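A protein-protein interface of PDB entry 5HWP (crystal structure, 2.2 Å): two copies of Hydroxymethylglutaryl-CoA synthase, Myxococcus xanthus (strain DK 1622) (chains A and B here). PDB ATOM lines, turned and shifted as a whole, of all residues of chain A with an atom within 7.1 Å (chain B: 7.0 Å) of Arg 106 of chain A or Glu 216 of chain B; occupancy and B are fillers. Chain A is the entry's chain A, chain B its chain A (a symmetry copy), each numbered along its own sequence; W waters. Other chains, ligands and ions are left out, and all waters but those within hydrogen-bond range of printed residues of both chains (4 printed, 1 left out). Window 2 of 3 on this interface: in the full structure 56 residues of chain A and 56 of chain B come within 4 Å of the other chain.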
ATOM      1  N   PRO A  74      39.747   8.274 -32.419  1.00  0.00           N
ATOM      2  CA  PRO A  74      38.374   8.165 -31.896  1.00  0.00           C
ATOM      3  C   PRO A  74      38.294   7.565 -30.505  1.00  0.00           C
ATOM      4  O   PRO A  74      37.357   7.882 -29.762  1.00  0.00           O
ATOM      5  CB  PRO A  74      37.669   7.277 -32.932  1.00  0.00           C
ATOM      6  CG  PRO A  74      38.482   7.397 -34.167  1.00  0.00           C
ATOM      7  CD  PRO A  74      39.896   7.586 -33.713  1.00  0.00           C
ATOM      8  N   SER A  75      39.242   6.709 -30.122  1.00  0.00           N
ATOM      9  CA  SER A  75      39.175   6.055 -28.822  1.00  0.00           C
ATOM     10  C   SER A  75      39.576   6.973 -27.676  1.00  0.00           C
ATOM     11  O   SER A  75      39.451   6.573 -26.514  1.00  0.00           O
ATOM     12  CB  SER A  75      40.057   4.804 -28.811  1.00  0.00           C
ATOM     13  OG  SER A  75      41.423   5.132 -28.984  1.00  0.00           O
ATOM     14  N   ILE A  77      38.018   9.897 -27.408  1.00  0.00           N
ATOM     15  CA  ILE A  77      36.806  10.678 -27.188  1.00  0.00           C
ATOM     16  C   ILE A  77      36.046  10.069 -26.015  1.00  0.00           C
ATOM     17  O   ILE A  77      35.608   8.916 -26.079  1.00  0.00           O
ATOM     18  CB  ILE A  77      35.933  10.719 -28.451  1.00  0.00           C
ATOM     19  CG1 ILE A  77      36.708  11.337 -29.619  1.00  0.00           C
ATOM     20  CG2 ILE A  77      34.652  11.511 -28.189  1.00  0.00           C
ATOM     21  CD1 ILE A  77      36.017  11.184 -30.962  1.00  0.00           C
ATOM     22  N   GLN A  99      27.356   8.830 -33.249  1.00  0.00           N
ATOM     23  CA  GLN A  99      28.263   7.775 -32.806  1.00  0.00           C
ATOM     24  C   GLN A  99      28.242   6.589 -33.765  1.00  0.00           C
ATOM     25  O   GLN A  99      29.293   6.059 -34.145  1.00  0.00           O
ATOM     26  CB  GLN A  99      27.884   7.327 -31.394  1.00  0.00           C
ATOM     27  CG  GLN A  99      28.822   6.298 -30.794  1.00  0.00           C
ATOM     28  CD  GLN A  99      28.404   5.882 -29.398  1.00  0.00           C
ATOM     29  OE1 GLN A  99      27.223   5.653 -29.133  1.00  0.00           O
ATOM     30  NE2 GLN A  99      29.369   5.789 -28.495  1.00  0.00           N
ATOM     31  N   LEU A 104      32.190   5.096 -34.008  1.00  0.00           N
ATOM     32  CA  LEU A 104      33.015   5.418 -32.858  1.00  0.00           C
ATOM     33  C   LEU A 104      32.956   4.294 -31.826  1.00  0.00           C
ATOM     34  O   LEU A 104      31.983   3.539 -31.770  1.00  0.00           O
ATOM     35  CB  LEU A 104      32.550   6.724 -32.218  1.00  0.00           C
ATOM     36  CG  LEU A 104      32.666   7.997 -33.059  1.00  0.00           C
ATOM     37  CD1 LEU A 104      32.107   9.179 -32.289  1.00  0.00           C
ATOM     38  CD2 LEU A 104      34.109   8.260 -33.459  1.00  0.00           C
ATOM     39  N   PRO A 105      33.995   4.164 -30.992  1.00  0.00           N
ATOM     40  CA  PRO A 105      33.963   3.141 -29.936  1.00  0.00           C
ATOM     41  C   PRO A 105      32.993   3.495 -28.817  1.00  0.00           C
ATOM     42  O   PRO A 105      32.219   4.451 -28.934  1.00  0.00           O
ATOM     43  CB  PRO A 105      35.418   3.086 -29.450  1.00  0.00           C
ATOM     44  CG  PRO A 105      36.001   4.401 -29.816  1.00  0.00           C
ATOM     45  CD  PRO A 105      35.291   4.863 -31.052  1.00  0.00           C
ATOM     46  N   ARG A 106      33.036   2.738 -27.720  1.00  0.00           N
ATOM     47  CA  ARG A 106      31.955   2.746 -26.743  1.00  0.00           C
ATOM     48  C   ARG A 106      32.250   3.535 -25.475  1.00  0.00           C
ATOM     49  O   ARG A 106      31.311   3.845 -24.735  1.00  0.00           O
ATOM     50  CB  ARG A 106      31.601   1.305 -26.356  1.00  0.00           C
ATOM     51  CG  ARG A 106      31.161   0.468 -27.540  1.00  0.00           C
ATOM     52  CD  ARG A 106      30.693  -0.912 -27.129  1.00  0.00           C
ATOM     53  NE  ARG A 106      29.848  -1.502 -28.162  1.00  0.00           N
ATOM     54  CZ  ARG A 106      29.154  -2.626 -28.020  1.00  0.00           C
ATOM     55  NH1 ARG A 106      29.199  -3.306 -26.882  1.00  0.00           N
ATOM     56  NH2 ARG A 106      28.412  -3.070 -29.026  1.00  0.00           N
ATOM     57  N   THR A 107      33.510   3.868 -25.198  1.00  0.00           N
ATOM     58  CA  THR A 107      33.874   4.490 -23.922  1.00  0.00           C
ATOM     59  C   THR A 107      33.706   6.008 -24.014  1.00  0.00           C
ATOM     60  O   THR A 107      34.667   6.780 -24.032  1.00  0.00           O
ATOM     61  CB  THR A 107      35.300   4.112 -23.536  1.00  0.00           C
ATOM     62  OG1 THR A 107      35.436   2.687 -23.551  1.00  0.00           O
ATOM     63  CG2 THR A 107      35.639   4.634 -22.142  1.00  0.00           C
ATOM     64  N   MET A 108      32.444   6.433 -24.056  1.00  0.00           N
ATOM     65  CA  MET A 108      32.149   7.857 -24.117  1.00  0.00           C
ATOM     66  C   MET A 108      30.711   8.102 -23.691  1.00  0.00           C
ATOM     67  O   MET A 108      29.822   7.285 -23.955  1.00  0.00           O
ATOM     68  CB  MET A 108      32.376   8.414 -25.527  1.00  0.00           C
ATOM     69  CG  MET A 108      31.445   7.823 -26.579  1.00  0.00           C
ATOM     70  SD  MET A 108      31.760   8.443 -28.241  1.00  0.00           S
ATOM     71  CE  MET A 108      33.377   7.747 -28.563  1.00  0.00           C
ATOM     72  N   ARG A 109      30.492   9.238 -23.033  1.00  0.00           N
ATOM     73  CA  ARG A 109      29.138   9.729 -22.835  1.00  0.00           C
ATOM     74  C   ARG A 109      28.588  10.254 -24.150  1.00  0.00           C
ATOM     75  O   ARG A 109      29.294  10.908 -24.921  1.00  0.00           O
ATOM     76  CB  ARG A 109      29.101  10.855 -21.802  1.00  0.00           C
ATOM     77  CG  ARG A 109      29.691  10.529 -20.455  1.00  0.00           C
ATOM     78  CD  ARG A 109      29.588  11.744 -19.553  1.00  0.00           C
ATOM     79  NE  ARG A 109      30.230  11.531 -18.262  1.00  0.00           N
ATOM     80  CZ  ARG A 109      30.716  12.501 -17.496  1.00  0.00           C
ATOM     81  NH1 ARG A 109      30.649  13.766 -17.888  1.00  0.00           N
ATOM     82  NH2 ARG A 109      31.280  12.204 -16.336  1.00  0.00           N
ATOM     83  N   THR A 110      27.319   9.970 -24.403  1.00  0.00           N
ATOM     84  CA  THR A 110      26.607  10.574 -25.516  1.00  0.00           C
ATOM     85  C   THR A 110      25.297  11.142 -24.995  1.00  0.00           C
ATOM     86  O   THR A 110      24.652  10.536 -24.136  1.00  0.00           O
ATOM     87  CB  THR A 110      26.351   9.559 -26.649  1.00  0.00           C
ATOM     88  OG1 THR A 110      25.507   8.502 -26.178  1.00  0.00           O
ATOM     89  CG2 THR A 110      27.662   8.962 -27.136  1.00  0.00           C
ATOM     90  N   VAL B 186      31.813   3.997 -18.534  1.00  0.00           N
ATOM     91  CA  VAL B 186      30.772   4.369 -19.485  1.00  0.00           C
ATOM     92  C   VAL B 186      30.862   3.466 -20.707  1.00  0.00           C
ATOM     93  O   VAL B 186      31.947   3.044 -21.116  1.00  0.00           O
ATOM     94  CB  VAL B 186      30.876   5.864 -19.875  1.00  0.00           C
ATOM     95  CG1 VAL B 186      32.076   6.122 -20.785  1.00  0.00           C
ATOM     96  CG2 VAL B 186      29.582   6.337 -20.517  1.00  0.00           C
ATOM     97  N   CYS B 187      29.703   3.184 -21.298  1.00  0.00           N
ATOM     98  CA  CYS B 187      29.612   2.290 -22.448  1.00  0.00           C
ATOM     99  C   CYS B 187      28.394   2.689 -23.265  1.00  0.00           C
ATOM    100  O   CYS B 187      27.273   2.666 -22.747  1.00  0.00           O
ATOM    101  CB  CYS B 187      29.512   0.830 -21.997  1.00  0.00           C
ATOM    102  SG  CYS B 187      29.366  -0.357 -23.354  1.00  0.00           S
ATOM    103  N   SER B 188      28.610   3.046 -24.532  1.00  0.00           N
ATOM    104  CA  SER B 188      27.545   3.553 -25.387  1.00  0.00           C
ATOM    105  C   SER B 188      27.696   3.000 -26.798  1.00  0.00           C
ATOM    106  O   SER B 188      28.801   2.694 -27.250  1.00  0.00           O
ATOM    107  CB  SER B 188      27.546   5.087 -25.432  1.00  0.00           C
ATOM    108  OG  SER B 188      28.772   5.580 -25.947  1.00  0.00           O
ATOM    109  N   MET B 189      26.565   2.881 -27.492  1.00  0.00           N
ATOM    110  CA  MET B 189      26.552   2.364 -28.853  1.00  0.00           C
ATOM    111  C   MET B 189      25.220   2.710 -29.501  1.00  0.00           C
ATOM    112  O   MET B 189      24.190   2.799 -28.827  1.00  0.00           O
ATOM    113  CB  MET B 189      26.778   0.847 -28.882  1.00  0.00           C
ATOM    114  CG  MET B 189      25.672   0.047 -28.218  1.00  0.00           C
ATOM    115  SD  MET B 189      26.268  -1.067 -26.931  1.00  0.00           S
ATOM    116  CE  MET B 189      27.005   0.086 -25.779  1.00  0.00           C
ATOM    117  N   ASP B 190      25.257   2.886 -30.819  1.00  0.00           N
ATOM    118  CA  ASP B 190      24.091   3.289 -31.598  1.00  0.00           C
ATOM    119  C   ASP B 190      23.167   2.089 -31.792  1.00  0.00           C
ATOM    120  O   ASP B 190      23.510   1.144 -32.509  1.00  0.00           O
ATOM    121  CB  ASP B 190      24.552   3.862 -32.937  1.00  0.00           C
ATOM    122  CG  ASP B 190      23.403   4.356 -33.794  1.00  0.00           C
ATOM    123  OD1 ASP B 190      22.326   4.646 -33.238  1.00  0.00           O
ATOM    124  OD2 ASP B 190      23.587   4.459 -35.027  1.00  0.00           O
ATOM    125  N   VAL B 191      21.990   2.124 -31.158  1.00  0.00           N
ATOM    126  CA  VAL B 191      21.040   1.018 -31.216  1.00  0.00           C
ATOM    127  C   VAL B 191      19.617   1.560 -31.275  1.00  0.00           C
ATOM    128  O   VAL B 191      19.335   2.690 -30.871  1.00  0.00           O
ATOM    129  CB  VAL B 191      21.178   0.059 -30.011  1.00  0.00           C
ATOM    130  CG1 VAL B 191      22.514  -0.665 -30.049  1.00  0.00           C
ATOM    131  CG2 VAL B 191      21.005   0.814 -28.695  1.00  0.00           C
ATOM    132  N   TYR B 209      15.024  -7.066 -26.574  1.00  0.00           N
ATOM    133  CA  TYR B 209      16.275  -6.524 -27.091  1.00  0.00           C
ATOM    134  C   TYR B 209      16.767  -5.353 -26.248  1.00  0.00           C
ATOM    135  O   TYR B 209      17.979  -5.184 -26.079  1.00  0.00           O
ATOM    136  CB  TYR B 209      16.089  -6.105 -28.550  1.00  0.00           C
ATOM    137  CG  TYR B 209      17.303  -5.466 -29.188  1.00  0.00           C
ATOM    138  CD1 TYR B 209      18.533  -6.115 -29.202  1.00  0.00           C
ATOM    139  CD2 TYR B 209      17.213  -4.223 -29.795  1.00  0.00           C
ATOM    140  CE1 TYR B 209      19.641  -5.531 -29.793  1.00  0.00           C
ATOM    141  CE2 TYR B 209      18.312  -3.632 -30.387  1.00  0.00           C
ATOM    142  CZ  TYR B 209      19.524  -4.288 -30.385  1.00  0.00           C
ATOM    143  OH  TYR B 209      20.617  -3.697 -30.977  1.00  0.00           O
ATOM    144  N   SER B 210      15.854  -4.546 -25.700  1.00  0.00           N
ATOM    145  CA  SER B 210      16.273  -3.472 -24.806  1.00  0.00           C
ATOM    146  C   SER B 210      16.863  -4.022 -23.515  1.00  0.00           C
ATOM    147  O   SER B 210      17.745  -3.392 -22.921  1.00  0.00           O
ATOM    148  CB  SER B 210      15.095  -2.544 -24.496  1.00  0.00           C
ATOM    149  OG  SER B 210      14.157  -3.168 -23.636  1.00  0.00           O
ATOM    150  N   ILE B 211      16.393  -5.186 -23.069  1.00  0.00           N
ATOM    151  CA  ILE B 211      16.983  -5.829 -21.898  1.00  0.00           C
ATOM    152  C   ILE B 211      18.420  -6.240 -22.191  1.00  0.00           C
ATOM    153  O   ILE B 211      19.326  -6.009 -21.381  1.00  0.00           O
ATOM    154  CB  ILE B 211      16.120  -7.029 -21.461  1.00  0.00           C
ATOM    155  CG1 ILE B 211      14.806  -6.525 -20.859  1.00  0.00           C
ATOM    156  CG2 ILE B 211      16.864  -7.915 -20.455  1.00  0.00           C
ATOM    157  CD1 ILE B 211      13.762  -7.604 -20.640  1.00  0.00           C
ATOM    158  N   THR B 212      18.651  -6.853 -23.354  1.00  0.00           N
ATOM    159  CA  THR B 212      20.004  -7.250 -23.734  1.00  0.00           C
ATOM    160  C   THR B 212      20.924  -6.039 -23.839  1.00  0.00           C
ATOM    161  O   THR B 212      22.046  -6.052 -23.320  1.00  0.00           O
ATOM    162  CB  THR B 212      19.965  -8.019 -25.058  1.00  0.00           C
ATOM    163  OG1 THR B 212      19.137  -9.180 -24.911  1.00  0.00           O
ATOM    164  CG2 THR B 212      21.362  -8.455 -25.487  1.00  0.00           C
ATOM    165  N   CYS B 213      20.465  -4.980 -24.513  1.00  0.00           N
ATOM    166  CA  CYS B 213      21.267  -3.762 -24.603  1.00  0.00           C
ATOM    167  C   CYS B 213      21.573  -3.204 -23.219  1.00  0.00           C
ATOM    168  O   CYS B 213      22.701  -2.777 -22.948  1.00  0.00           O
ATOM    169  CB  CYS B 213      20.544  -2.717 -25.452  1.00  0.00           C
ATOM    170  SG  CYS B 213      20.386  -3.155 -27.200  1.00  0.00           S
ATOM    171  N   TYR B 214      20.576  -3.195 -22.332  1.00  0.00           N
ATOM    172  CA  TYR B 214      20.796  -2.772 -20.952  1.00  0.00           C
ATOM    173  C   TYR B 214      21.953  -3.543 -20.329  1.00  0.00           C
ATOM    174  O   TYR B 214      22.906  -2.949 -19.810  1.00  0.00           O
ATOM    175  CB  TYR B 214      19.504  -2.972 -20.151  1.00  0.00           C
ATOM    176  CG  TYR B 214      19.532  -2.508 -18.705  1.00  0.00           C
ATOM    177  CD1 TYR B 214      20.357  -3.120 -17.766  1.00  0.00           C
ATOM    178  CD2 TYR B 214      18.695  -1.489 -18.269  1.00  0.00           C
ATOM    179  CE1 TYR B 214      20.370  -2.709 -16.446  1.00  0.00           C
ATOM    180  CE2 TYR B 214      18.699  -1.072 -16.948  1.00  0.00           C
ATOM    181  CZ  TYR B 214      19.539  -1.687 -16.042  1.00  0.00           C
ATOM    182  OH  TYR B 214      19.550  -1.281 -14.727  1.00  0.00           O
ATOM    183  N   LEU B 215      21.890  -4.875 -20.379  1.00  0.00           N
ATOM    184  CA  LEU B 215      22.905  -5.694 -19.727  1.00  0.00           C
ATOM    185  C   LEU B 215      24.256  -5.594 -20.425  1.00  0.00           C
ATOM    186  O   LEU B 215      25.297  -5.667 -19.762  1.00  0.00           O
ATOM    187  CB  LEU B 215      22.437  -7.148 -19.667  1.00  0.00           C
ATOM    188  CG  LEU B 215      21.161  -7.379 -18.851  1.00  0.00           C
ATOM    189  CD1 LEU B 215      20.700  -8.820 -18.976  1.00  0.00           C
ATOM    190  CD2 LEU B 215      21.365  -7.013 -17.386  1.00  0.00           C
ATOM    191  N   GLU B 216      24.272  -5.432 -21.750  1.00  0.00           N
ATOM    192  CA  GLU B 216      25.542  -5.251 -22.445  1.00  0.00           C
ATOM    193  C   GLU B 216      26.189  -3.928 -22.051  1.00  0.00           C
ATOM    194  O   GLU B 216      27.376  -3.884 -21.703  1.00  0.00           O
ATOM    195  CB  GLU B 216      25.339  -5.317 -23.960  1.00  0.00           C
ATOM    196  CG  GLU B 216      26.641  -5.248 -24.751  1.00  0.00           C
ATOM    197  CD  GLU B 216      26.423  -5.330 -26.250  1.00  0.00           C
ATOM    198  OE1 GLU B 216      25.256  -5.253 -26.690  1.00  0.00           O
ATOM    199  OE2 GLU B 216      27.420  -5.474 -26.989  1.00  0.00           O
ATOM    200  N   ALA B 217      25.424  -2.838 -22.100  1.00  0.00           N
ATOM    201  CA  ALA B 217      25.968  -1.539 -21.720  1.00  0.00           C
ATOM    202  C   ALA B 217      26.349  -1.513 -20.246  1.00  0.00           C
ATOM    203  O   ALA B 217      27.370  -0.927 -19.870  1.00  0.00           O
ATOM    204  CB  ALA B 217      24.959  -0.437 -22.036  1.00  0.00           C
ATOM    205  N   LEU B 218      25.537  -2.145 -19.393  1.00  0.00           N
ATOM    206  CA  LEU B 218      25.881  -2.256 -17.980  1.00  0.00           C
ATOM    207  C   LEU B 218      27.257  -2.885 -17.803  1.00  0.00           C
ATOM    208  O   LEU B 218      28.092  -2.384 -17.040  1.00  0.00           O
ATOM    209  CB  LEU B 218      24.818  -3.079 -17.246  1.00  0.00           C
ATOM    210  CG  LEU B 218      25.044  -3.395 -15.761  1.00  0.00           C
ATOM    211  CD1 LEU B 218      23.708  -3.683 -15.097  1.00  0.00           C
ATOM    212  CD2 LEU B 218      25.983  -4.583 -15.516  1.00  0.00           C
ATOM    213  N   SER B 219      27.503  -3.997 -18.497  1.00  0.00           N
ATOM    214  CA  SER B 219      28.754  -4.729 -18.316  1.00  0.00           C
ATOM    215  C   SER B 219      29.953  -3.849 -18.642  1.00  0.00           C
ATOM    216  O   SER B 219      30.940  -3.821 -17.899  1.00  0.00           O
ATOM    217  CB  SER B 219      28.753  -5.985 -19.189  1.00  0.00           C
ATOM    218  OG  SER B 219      27.652  -6.819 -18.876  1.00  0.00           O
ATOM    219  N   GLY B 220      29.888  -3.127 -19.761  1.00  0.00           N
ATOM    220  CA  GLY B 220      30.986  -2.246 -20.120  1.00  0.00           C
ATOM    221  C   GLY B 220      31.171  -1.120 -19.124  1.00  0.00           C
ATOM    222  O   GLY B 220      32.296  -0.808 -18.726  1.00  0.00           O
ATOM    223  N   ALA B 221      30.069  -0.500 -18.699  1.00  0.00           N
ATOM    224  CA  ALA B 221      30.158   0.616 -17.762  1.00  0.00           C
ATOM    225  C   ALA B 221      30.728   0.161 -16.425  1.00  0.00           C
ATOM    226  O   ALA B 221      31.619   0.812 -15.866  1.00  0.00           O
ATOM    227  CB  ALA B 221      28.780   1.254 -17.577  1.00  0.00           C
ATOM    228  N   ARG B 223      32.598  -2.518 -15.763  1.00  0.00           N
ATOM    229  CA  ARG B 223      33.999  -2.892 -15.918  1.00  0.00           C
ATOM    230  C   ARG B 223      34.888  -1.658 -16.000  1.00  0.00           C
ATOM    231  O   ARG B 223      35.968  -1.621 -15.400  1.00  0.00           O
ATOM    232  CB  ARG B 223      34.181  -3.767 -17.157  1.00  0.00           C
ATOM    233  CG  ARG B 223      33.687  -5.194 -16.988  1.00  0.00           C
ATOM    234  CD  ARG B 223      33.899  -6.000 -18.260  1.00  0.00           C
ATOM    235  NE  ARG B 223      33.848  -7.441 -18.027  1.00  0.00           N
ATOM    236  CZ  ARG B 223      32.914  -8.264 -18.496  1.00  0.00           C
ATOM    237  NH1 ARG B 223      31.922  -7.815 -19.249  1.00  0.00           N
ATOM    238  NH2 ARG B 223      32.979  -9.560 -18.217  1.00  0.00           N
ATOM    239  N   GLN B 265      24.006  -9.788 -13.650  1.00  0.00           N
ATOM    240  CA  GLN B 265      24.973  -9.505 -14.703  1.00  0.00           C
ATOM    241  C   GLN B 265      26.226  -8.848 -14.136  1.00  0.00           C
ATOM    242  O   GLN B 265      27.346  -9.230 -14.490  1.00  0.00           O
ATOM    243  CB  GLN B 265      24.333  -8.618 -15.772  1.00  0.00           C
ATOM    244  CG  GLN B 265      25.255  -8.259 -16.926  1.00  0.00           C
ATOM    245  CD  GLN B 265      25.733  -9.475 -17.694  1.00  0.00           C
ATOM    246  OE1 GLN B 265      24.998 -10.034 -18.506  1.00  0.00           O
ATOM    247  NE2 GLN B 265      26.966  -9.893 -17.436  1.00  0.00           N
ATOM    248  N   TYR B 342      21.265   3.756 -17.072  1.00  0.00           N
ATOM    249  CA  TYR B 342      21.134   3.304 -18.447  1.00  0.00           C
ATOM    250  C   TYR B 342      20.195   4.222 -19.212  1.00  0.00           C
ATOM    251  O   TYR B 342      19.218   4.746 -18.665  1.00  0.00           O
ATOM    252  CB  TYR B 342      20.605   1.868 -18.531  1.00  0.00           C
ATOM    253  CG  TYR B 342      20.430   1.394 -19.955  1.00  0.00           C
ATOM    254  CD1 TYR B 342      21.530   1.076 -20.737  1.00  0.00           C
ATOM    255  CD2 TYR B 342      19.168   1.275 -20.521  1.00  0.00           C
ATOM    256  CE1 TYR B 342      21.380   0.649 -22.043  1.00  0.00           C
ATOM    257  CE2 TYR B 342      19.008   0.847 -21.826  1.00  0.00           C
ATOM    258  CZ  TYR B 342      20.119   0.536 -22.581  1.00  0.00           C
ATOM    259  OH  TYR B 342      19.966   0.110 -23.880  1.00  0.00           O
ATOM    260  N   CYS B 346      22.182   3.851 -27.345  1.00  0.00           N
ATOM    261  CA  CYS B 346      22.051   3.728 -25.896  1.00  0.00           C
ATOM    262  C   CYS B 346      23.318   4.206 -25.209  1.00  0.00           C
ATOM    263  O   CYS B 346      24.327   4.488 -25.861  1.00  0.00           O
ATOM    264  CB  CYS B 346      21.772   2.273 -25.496  1.00  0.00           C
ATOM    265  SG  CYS B 346      23.215   1.187 -25.645  1.00  0.00           S
ATOM    266  N   ALA B 348      25.281   3.704 -21.060  1.00  0.00           N
ATOM    267  CA  ALA B 348      25.278   3.359 -19.650  1.00  0.00           C
ATOM    268  C   ALA B 348      26.485   3.992 -18.980  1.00  0.00           C
ATOM    269  O   ALA B 348      27.553   4.121 -19.582  1.00  0.00           O
ATOM    270  CB  ALA B 348      25.302   1.843 -19.430  1.00  0.00           C
HETATM  271  O   HOH W   1      30.797  -3.394 -24.426  1.00  0.00           O
HETATM  272  O   HOH W   2      24.928   6.280 -27.777  1.00  0.00           O
HETATM  273  O   HOH W   3      25.813  -4.624 -29.444  1.00  0.00           O
HETATM  274  O   HOH W   4      32.968   1.059 -22.683  1.00  0.00           O
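NE2 of Gln 99 of chain A is in hydrogen-bond range of OG of Ser 188 of chain B (2.6 Å). OE1 of Gln 99 of chain A is in hydrogen-bond range of N of Met 189 of chain B, 3.3 Å away. The backbone NH (N) of Ser 188 of chain B is in hydrogen-bond range of the backbone carbonyl oxygen (O) of Arg 106 of chain A (2.8 Å). SD of Met 189 of chain B sits close to NH2 of Arg 106 of chain A, 3.6 Å away. NH1 of Arg 106 of chain A lies within salt-bridge range of OE2 of Glu 216 of chain B (2.8 Å). The backbone carbonyl oxygen of Met 108 of chain A is in hydrogen-bond range of the side-chain hydroxyl of Ser 188 of chain B.
The backbone carbonyl oxygen (O) of Gln 99 of chain A is in hydrogen-bond range of the backbone NH (N) of Leu 104 of chain A (3.1 Å). NE2 of Gln 99 of chain A sits at hydrogen-bond distance from O of Pro 105 of chain A. The side-chain sulfur (SD) of Met 108 of chain A sits close to the side-chain amide nitrogen (NE2) of Gln 99 of chain A, at 3.6 Å. The backbone NH (N) of Ala 348 of chain B sits at hydrogen-bond distance from the backbone carbonyl oxygen (O) of Cys 187 of chain B (2.8 Å). The backbone NH (N) of Cys 346 of chain B lies within hydrogen-bond range of the backbone carbonyl oxygen (O) of Met 189 of chain B, at 2.7 Å.
Asp 190 of chain B touches Gln 99 of chain A (N to OE1, 3.8 Å). Arg 106 of chain A touches Val 186 of chain B. Arg 106 of chain A touches Cys 187 of chain B (O to CA, 3.2 Å). Val 186 of chain B touches Thr 107 of chain A (CG1 to C, 3.6 Å). Met 108 of chain A touches Val 186 of chain B. CG2 of Val 186 of chain B touches N of Arg 109 of chain A (3.9 Å). Ser 188 of chain B touches Thr 110 of chain A (OG to CG2, 3.8 Å).
Of chain B, only Val 186 (3.8 Å), Cys 187 (3.2 Å), Ser 188 (2.8 Å), Met 189 (3.5 Å) and Glu 216 (2.8 Å) come within 4 Å of Arg 106 of chain A. Printed residues of chain A within 4 Å of Glu 216 of chain B: Arg 106. Printed residues of chain B within 4 Å of Arg 109 of chain A: Val 186 (3.9 Å). Printed residues of chain B within 4 Å of Met 108 of chain A: Val 186 (3.3 Å) and Ser 188 (2.8 Å). Printed residues of chain A within 4 Å of Asp 190 of chain B: Gln 99. Of the printed residues of chain A, Cys 187 of chain B touches Arg 106. Of the printed residues of chain B, Thr 107 of chain A touches Val 186. The nearest residue of chain B that does not touch Arg 106 of chain A is Ala 217 of chain B (6.1 Å).
Of the 24 printed residues of chain B, 6 touch a printed residue of chain A. Hydrophobic or aromatic side chains of chain B that line the printed part of chain A: Val 186 and Met 189. Of the 11 printed residues of chain A, 6 touch a printed residue of chain B. Printed residues of chain A that touch a printed residue of chain B: Gln 99, Arg 106, Thr 107, Met 108, Arg 109 and Thr 110. Along chain A the printed residues that touch a printed residue of chain B span positions 99 to 110. Among the printed residues, 13 pairs touch across the chains.
No position is printed for both chains.
Water W2 lies within hydrogen-bond range of the backbone carbonyl oxygen of Cys 346 of chain B (2.7 Å), the side-chain amide oxygen of Gln 99 of chain A (2.7 Å) and the side-chain hydroxyl of Thr 110 of chain A (2.8 Å). Water W4 bridges the backbone carbonyl oxygen (O) of Val 186 of chain B (2.7 Å) and the side-chain hydroxyl (OG1) of Thr 107 of chain A (3.1 Å). Water W3 bridges the side-chain carboxylate of Glu 216 of chain B and the guanidinium group of Arg 106 of chain A. Water W1 lies within hydrogen-bond range of NH1 of Arg 106 of chain A and SG of Cys 187 of chain B.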
